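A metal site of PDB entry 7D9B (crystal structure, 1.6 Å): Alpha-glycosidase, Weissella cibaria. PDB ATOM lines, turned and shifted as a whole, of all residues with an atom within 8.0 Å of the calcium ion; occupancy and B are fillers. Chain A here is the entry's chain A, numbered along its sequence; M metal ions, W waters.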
ATOM      1  N   PRO A 150     -37.487   0.108 -11.407  1.00  0.00           N
ATOM      2  CA  PRO A 150     -36.490   0.732 -12.312  1.00  0.00           C
ATOM      3  C   PRO A 150     -35.689  -0.252 -13.143  1.00  0.00           C
ATOM      4  O   PRO A 150     -35.240   0.098 -14.233  1.00  0.00           O
ATOM      5  CB  PRO A 150     -35.578   1.506 -11.361  1.00  0.00           C
ATOM      6  CG  PRO A 150     -36.359   1.746 -10.215  1.00  0.00           C
ATOM      7  CD  PRO A 150     -37.296   0.553 -10.013  1.00  0.00           C
ATOM      8  N   GLU A 151     -35.478  -1.472 -12.663  1.00  0.00           N
ATOM      9  CA  GLU A 151     -34.719  -2.439 -13.472  1.00  0.00           C
ATOM     10  C   GLU A 151     -35.418  -2.739 -14.786  1.00  0.00           C
ATOM     11  O   GLU A 151     -34.785  -3.272 -15.707  1.00  0.00           O
ATOM     12  CB  GLU A 151     -34.533  -3.769 -12.707  1.00  0.00           C
ATOM     13  CG  GLU A 151     -33.078  -4.309 -12.708  1.00  0.00           C
ATOM     14  CD  GLU A 151     -32.689  -4.982 -14.025  1.00  0.00           C
ATOM     15  OE1 GLU A 151     -31.604  -4.660 -14.567  1.00  0.00           O
ATOM     16  OE2 GLU A 151     -33.462  -5.866 -14.526  1.00  0.00           O
ATOM     17  N   ALA A 154     -36.714   1.322 -18.480  1.00  0.00           N
ATOM     18  CA  ALA A 154     -35.979   1.604 -19.699  1.00  0.00           C
ATOM     19  C   ALA A 154     -34.481   1.552 -19.415  1.00  0.00           C
ATOM     20  O   ALA A 154     -34.026   2.029 -18.372  1.00  0.00           O
ATOM     21  CB  ALA A 154     -36.364   2.984 -20.287  1.00  0.00           C
ATOM     22  N   ASN A 155     -33.716   0.951 -20.327  1.00  0.00           N
ATOM     23  CA  ASN A 155     -32.262   0.962 -20.238  1.00  0.00           C
ATOM     24  C   ASN A 155     -31.775   2.197 -20.984  1.00  0.00           C
ATOM     25  O   ASN A 155     -31.717   2.214 -22.207  1.00  0.00           O
ATOM     26  CB  ASN A 155     -31.684  -0.310 -20.852  1.00  0.00           C
ATOM     27  CG  ASN A 155     -30.194  -0.464 -20.593  1.00  0.00           C
ATOM     28  OD1 ASN A 155     -29.556   0.385 -19.962  1.00  0.00           O
ATOM     29  ND2 ASN A 155     -29.636  -1.580 -21.064  1.00  0.00           N
ATOM     30  N   GLY A 156     -31.407   3.240 -20.246  1.00  0.00           N
ATOM     31  CA  GLY A 156     -30.879   4.428 -20.871  1.00  0.00           C
ATOM     32  C   GLY A 156     -29.367   4.459 -20.946  1.00  0.00           C
ATOM     33  O   GLY A 156     -28.778   5.427 -21.470  1.00  0.00           O
ATOM     34  N   ASP A 157     -28.708   3.396 -20.485  1.00  0.00           N
ATOM     35  CA  ASP A 157     -27.246   3.397 -20.436  1.00  0.00           C
ATOM     36  C   ASP A 157     -26.766   1.948 -20.354  1.00  0.00           C
ATOM     37  O   ASP A 157     -26.822   1.341 -19.281  1.00  0.00           O
ATOM     38  CB  ASP A 157     -26.761   4.239 -19.262  1.00  0.00           C
ATOM     39  CG  ASP A 157     -25.272   4.386 -19.207  1.00  0.00           C
ATOM     40  OD1 ASP A 157     -24.568   3.768 -20.033  1.00  0.00           O
ATOM     41  OD2 ASP A 157     -24.781   5.132 -18.319  1.00  0.00           O
ATOM     42  N   VAL A 158     -26.295   1.383 -21.481  1.00  0.00           N
ATOM     43  CA  VAL A 158     -25.805   0.005 -21.389  1.00  0.00           C
ATOM     44  C   VAL A 158     -24.520  -0.092 -20.550  1.00  0.00           C
ATOM     45  O   VAL A 158     -24.163  -1.190 -20.101  1.00  0.00           O
ATOM     46  CB  VAL A 158     -25.500  -0.623 -22.768  1.00  0.00           C
ATOM     47  CG1 VAL A 158     -26.813  -0.794 -23.574  1.00  0.00           C
ATOM     48  CG2 VAL A 158     -24.472   0.231 -23.556  1.00  0.00           C
ATOM     49  N   SER A 159     -23.802   1.010 -20.358  1.00  0.00           N
ATOM     50  CA  SER A 159     -22.486   0.911 -19.730  1.00  0.00           C
ATOM     51  C   SER A 159     -22.573   0.612 -18.240  1.00  0.00           C
ATOM     52  O   SER A 159     -21.568   0.197 -17.651  1.00  0.00           O
ATOM     53  CB  SER A 159     -21.672   2.207 -19.984  1.00  0.00           C
ATOM     54  OG  SER A 159     -22.133   3.279 -19.172  1.00  0.00           O
ATOM     55  N   ASN A 160     -23.750   0.759 -17.619  1.00  0.00           N
ATOM     56  CA  ASN A 160     -23.868   0.409 -16.222  1.00  0.00           C
ATOM     57  C   ASN A 160     -24.603  -0.907 -16.036  1.00  0.00           C
ATOM     58  O   ASN A 160     -24.983  -1.227 -14.913  1.00  0.00           O
ATOM     59  CB  ASN A 160     -24.565   1.537 -15.441  1.00  0.00           C
ATOM     60  CG  ASN A 160     -25.989   1.825 -15.944  1.00  0.00           C
ATOM     61  OD1 ASN A 160     -26.623   0.952 -16.571  1.00  0.00           O
ATOM     62  ND2 ASN A 160     -26.503   3.031 -15.649  1.00  0.00           N
ATOM     63  N   ASP A 161     -24.788  -1.680 -17.097  1.00  0.00           N
ATOM     64  CA  ASP A 161     -25.620  -2.879 -16.986  1.00  0.00           C
ATOM     65  C   ASP A 161     -24.947  -3.943 -16.119  1.00  0.00           C
ATOM     66  O   ASP A 161     -23.718  -4.121 -16.201  1.00  0.00           O
ATOM     67  CB  ASP A 161     -25.898  -3.494 -18.370  1.00  0.00           C
ATOM     68  CG  ASP A 161     -26.890  -2.680 -19.193  1.00  0.00           C
ATOM     69  OD1 ASP A 161     -27.455  -1.710 -18.659  1.00  0.00           O
ATOM     70  OD2 ASP A 161     -27.074  -3.045 -20.374  1.00  0.00           O
ATOM     71  N   PRO A 162     -25.718  -4.707 -15.348  1.00  0.00           N
ATOM     72  CA  PRO A 162     -25.157  -5.834 -14.599  1.00  0.00           C
ATOM     73  C   PRO A 162     -24.572  -6.882 -15.526  1.00  0.00           C
ATOM     74  O   PRO A 162     -24.969  -6.999 -16.685  1.00  0.00           O
ATOM     75  CB  PRO A 162     -26.388  -6.403 -13.859  1.00  0.00           C
ATOM     76  CG  PRO A 162     -27.332  -5.207 -13.757  1.00  0.00           C
ATOM     77  CD  PRO A 162     -27.124  -4.407 -15.014  1.00  0.00           C
ATOM     78  N   THR A 165     -26.719  -9.203 -18.231  1.00  0.00           N
ATOM     79  CA  THR A 165     -27.937  -8.525 -18.686  1.00  0.00           C
ATOM     80  C   THR A 165     -28.452  -9.158 -19.979  1.00  0.00           C
ATOM     81  O   THR A 165     -27.683  -9.399 -20.929  1.00  0.00           O
ATOM     82  CB  THR A 165     -27.656  -7.031 -18.879  1.00  0.00           C
ATOM     83  OG1 THR A 165     -27.415  -6.425 -17.579  1.00  0.00           O
ATOM     84  CG2 THR A 165     -28.862  -6.314 -19.553  1.00  0.00           C
ATOM     85  N   TRP A 168     -33.510  -6.748 -24.214  1.00  0.00           N
ATOM     86  CA  TRP A 168     -34.764  -6.149 -23.747  1.00  0.00           C
ATOM     87  C   TRP A 168     -35.916  -6.765 -24.532  1.00  0.00           C
ATOM     88  O   TRP A 168     -36.089  -6.483 -25.716  1.00  0.00           O
ATOM     89  CB  TRP A 168     -34.717  -4.635 -23.946  1.00  0.00           C
ATOM     90  CG  TRP A 168     -35.800  -3.912 -23.189  1.00  0.00           C
ATOM     91  CD1 TRP A 168     -37.101  -3.707 -23.565  1.00  0.00           C
ATOM     92  CD2 TRP A 168     -35.650  -3.329 -21.899  1.00  0.00           C
ATOM     93  NE1 TRP A 168     -37.764  -3.005 -22.564  1.00  0.00           N
ATOM     94  CE2 TRP A 168     -36.890  -2.758 -21.533  1.00  0.00           C
ATOM     95  CE3 TRP A 168     -34.563  -3.227 -21.002  1.00  0.00           C
ATOM     96  CZ2 TRP A 168     -37.101  -2.091 -20.315  1.00  0.00           C
ATOM     97  CZ3 TRP A 168     -34.757  -2.592 -19.783  1.00  0.00           C
ATOM     98  CH2 TRP A 168     -36.025  -2.010 -19.447  1.00  0.00           C
ATOM     99  N   TYR A 180     -32.202  -6.858 -16.866  1.00  0.00           N
ATOM    100  CA  TYR A 180     -32.426  -6.281 -18.181  1.00  0.00           C
ATOM    101  C   TYR A 180     -31.803  -4.907 -18.349  1.00  0.00           C
ATOM    102  O   TYR A 180     -31.804  -4.383 -19.479  1.00  0.00           O
ATOM    103  CB  TYR A 180     -33.950  -6.211 -18.475  1.00  0.00           C
ATOM    104  CG  TYR A 180     -34.541  -7.579 -18.710  1.00  0.00           C
ATOM    105  CD1 TYR A 180     -35.033  -8.331 -17.634  1.00  0.00           C
ATOM    106  CD2 TYR A 180     -34.556  -8.144 -19.983  1.00  0.00           C
ATOM    107  CE1 TYR A 180     -35.582  -9.586 -17.837  1.00  0.00           C
ATOM    108  CE2 TYR A 180     -35.069  -9.406 -20.192  1.00  0.00           C
ATOM    109  CZ  TYR A 180     -35.583 -10.117 -19.125  1.00  0.00           C
ATOM    110  OH  TYR A 180     -36.104 -11.358 -19.375  1.00  0.00           O
ATOM    111  N   GLY A 181     -31.234  -4.330 -17.286  1.00  0.00           N
ATOM    112  CA  GLY A 181     -30.449  -3.111 -17.453  1.00  0.00           C
ATOM    113  C   GLY A 181     -31.206  -1.822 -17.296  1.00  0.00           C
ATOM    114  O   GLY A 181     -30.645  -0.751 -17.597  1.00  0.00           O
ATOM    115  N   GLY A 182     -32.455  -1.853 -16.828  1.00  0.00           N
ATOM    116  CA  GLY A 182     -33.174  -0.595 -16.625  1.00  0.00           C
ATOM    117  C   GLY A 182     -32.467   0.288 -15.612  1.00  0.00           C
ATOM    118  O   GLY A 182     -31.809  -0.195 -14.681  1.00  0.00           O
ATOM    119  N   ASP A 183     -32.561   1.611 -15.798  1.00  0.00           N
ATOM    120  CA  ASP A 183     -31.784   2.520 -14.948  1.00  0.00           C
ATOM    121  C   ASP A 183     -32.433   3.909 -14.911  1.00  0.00           C
ATOM    122  O   ASP A 183     -33.474   4.153 -15.520  1.00  0.00           O
ATOM    123  CB  ASP A 183     -30.316   2.608 -15.439  1.00  0.00           C
ATOM    124  CG  ASP A 183     -30.230   2.880 -16.937  1.00  0.00           C
ATOM    125  OD1 ASP A 183     -31.067   3.652 -17.460  1.00  0.00           O
ATOM    126  OD2 ASP A 183     -29.330   2.356 -17.619  1.00  0.00           O
ATOM    127  N   LEU A 184     -31.813   4.805 -14.141  1.00  0.00           N
ATOM    128  CA  LEU A 184     -32.356   6.161 -13.991  1.00  0.00           C
ATOM    129  C   LEU A 184     -32.298   6.946 -15.300  1.00  0.00           C
ATOM    130  O   LEU A 184     -33.185   7.764 -15.560  1.00  0.00           O
ATOM    131  CB  LEU A 184     -31.602   6.960 -12.907  1.00  0.00           C
ATOM    132  CG  LEU A 184     -31.642   6.402 -11.498  1.00  0.00           C
ATOM    133  CD1 LEU A 184     -30.963   7.419 -10.531  1.00  0.00           C
ATOM    134  CD2 LEU A 184     -33.105   6.100 -11.082  1.00  0.00           C
ATOM    135  N   GLN A 185     -31.254   6.729 -16.130  1.00  0.00           N
ATOM    136  CA  GLN A 185     -31.233   7.443 -17.396  1.00  0.00           C
ATOM    137  C   GLN A 185     -32.427   7.039 -18.257  1.00  0.00           C
ATOM    138  O   GLN A 185     -32.958   7.881 -19.001  1.00  0.00           O
ATOM    139  CB  GLN A 185     -29.925   7.185 -18.132  1.00  0.00           C
ATOM    140  CG  GLN A 185     -29.817   7.997 -19.437  1.00  0.00           C
ATOM    141  CD  GLN A 185     -29.837   9.501 -19.171  1.00  0.00           C
ATOM    142  OE1 GLN A 185     -29.040  10.014 -18.388  1.00  0.00           O
ATOM    143  NE2 GLN A 185     -30.717  10.207 -19.857  1.00  0.00           N
ATOM    144  N   GLY A 186     -32.872   5.776 -18.163  1.00  0.00           N
ATOM    145  CA  GLY A 186     -34.030   5.353 -18.948  1.00  0.00           C
ATOM    146  C   GLY A 186     -35.307   6.063 -18.522  1.00  0.00           C
ATOM    147  O   GLY A 186     -36.166   6.417 -19.364  1.00  0.00           O
ATOM    148  N   PRO A 226     -25.155   1.727  -8.331  1.00  0.00           N
ATOM    149  CA  PRO A 226     -24.401   2.196  -9.511  1.00  0.00           C
ATOM    150  C   PRO A 226     -24.865   1.603 -10.821  1.00  0.00           C
ATOM    151  O   PRO A 226     -24.529   2.150 -11.880  1.00  0.00           O
ATOM    152  CB  PRO A 226     -22.947   1.829  -9.182  1.00  0.00           C
ATOM    153  CG  PRO A 226     -23.010   0.845  -8.138  1.00  0.00           C
ATOM    154  CD  PRO A 226     -24.272   1.110  -7.313  1.00  0.00           C
ATOM    155  N   HIS A 227     -25.656   0.521 -10.805  1.00  0.00           N
ATOM    156  CA  HIS A 227     -26.254   0.022 -12.041  1.00  0.00           C
ATOM    157  C   HIS A 227     -27.445   0.859 -12.460  1.00  0.00           C
ATOM    158  O   HIS A 227     -27.889   0.738 -13.598  1.00  0.00           O
ATOM    159  CB  HIS A 227     -26.686  -1.427 -11.849  1.00  0.00           C
ATOM    160  CG  HIS A 227     -25.554  -2.329 -11.476  1.00  0.00           C
ATOM    161  ND1 HIS A 227     -25.312  -2.695 -10.174  1.00  0.00           N
ATOM    162  CD2 HIS A 227     -24.575  -2.904 -12.219  1.00  0.00           C
ATOM    163  CE1 HIS A 227     -24.229  -3.448 -10.126  1.00  0.00           C
ATOM    164  NE2 HIS A 227     -23.763  -3.595 -11.357  1.00  0.00           N
ATOM    165  N   PHE A 228     -27.953   1.673 -11.554  1.00  0.00           N
ATOM    166  CA  PHE A 228     -29.031   2.612 -11.842  1.00  0.00           C
ATOM    167  C   PHE A 228     -28.543   4.016 -12.133  1.00  0.00           C
ATOM    168  O   PHE A 228     -29.160   4.740 -12.937  1.00  0.00           O
ATOM    169  CB  PHE A 228     -30.019   2.678 -10.657  1.00  0.00           C
ATOM    170  CG  PHE A 228     -30.926   1.480 -10.515  1.00  0.00           C
ATOM    171  CD1 PHE A 228     -31.081   0.541 -11.545  1.00  0.00           C
ATOM    172  CD2 PHE A 228     -31.638   1.326  -9.330  1.00  0.00           C
ATOM    173  CE1 PHE A 228     -31.952  -0.565 -11.347  1.00  0.00           C
ATOM    174  CE2 PHE A 228     -32.529   0.229  -9.132  1.00  0.00           C
ATOM    175  CZ  PHE A 228     -32.664  -0.718 -10.162  1.00  0.00           C
ATOM    176  N   GLY A 229     -27.490   4.453 -11.449  1.00  0.00           N
ATOM    177  CA  GLY A 229     -27.022   5.809 -11.680  1.00  0.00           C
ATOM    178  C   GLY A 229     -26.180   6.278 -10.502  1.00  0.00           C
ATOM    179  O   GLY A 229     -25.567   5.471  -9.809  1.00  0.00           O
HETATM  180 CA    CA M   1     -28.398   0.235 -17.892  1.00  0.00          CA
HETATM  181  O   HOH W   1     -28.479  -0.883 -15.659  1.00  0.00           O
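The calcium ion is bound by OD1 of Asp 161, at 2.3 Å. OD1 of Asn 160 binds the calcium ion (2.3 Å). OD2 of Asp 183 binds the calcium ion (2.3 Å). The backbone carbonyl oxygen (O) of Asp 157 binds the calcium ion. The calcium ion is bound by the side-chain amide oxygen (OD1) of Asn 155. The calcium ion is bound by O of Gly 181. Water W1 binds the calcium ion, 2.5 Å away. The calcium ion has seven donor atoms within binding distance.
The side-chain carboxylate (OD1) of Asp 183 sits close to the backbone NH (N) of Gln 185 (3.4 Å). N of Gly 181 sits at hydrogen-bond distance from OE1 of Glu 151, at 2.8 Å. OG of Ser 159 sits at hydrogen-bond distance from OD1 of Asp 157. The side-chain carboxylate (OD1) of Asp 183 sits at hydrogen-bond distance from the backbone NH (N) of Gly 186. O of Ala 154 sits at hydrogen-bond distance from N of Asp 183 (3.0 Å). O of Pro 150 lies within hydrogen-bond range of N of Asp 183 (3.5 Å). The side-chain carboxylate of Asp 183 is in hydrogen-bond range of the backbone NH of Gly 156, at 2.8 Å. ND2 of Asn 160 lies close to O of His 227.
Within 4 Å of the calcium ion: Asn 155, Asp 157, Asn 160, Asp 161, Gly 181 and Asp 183.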
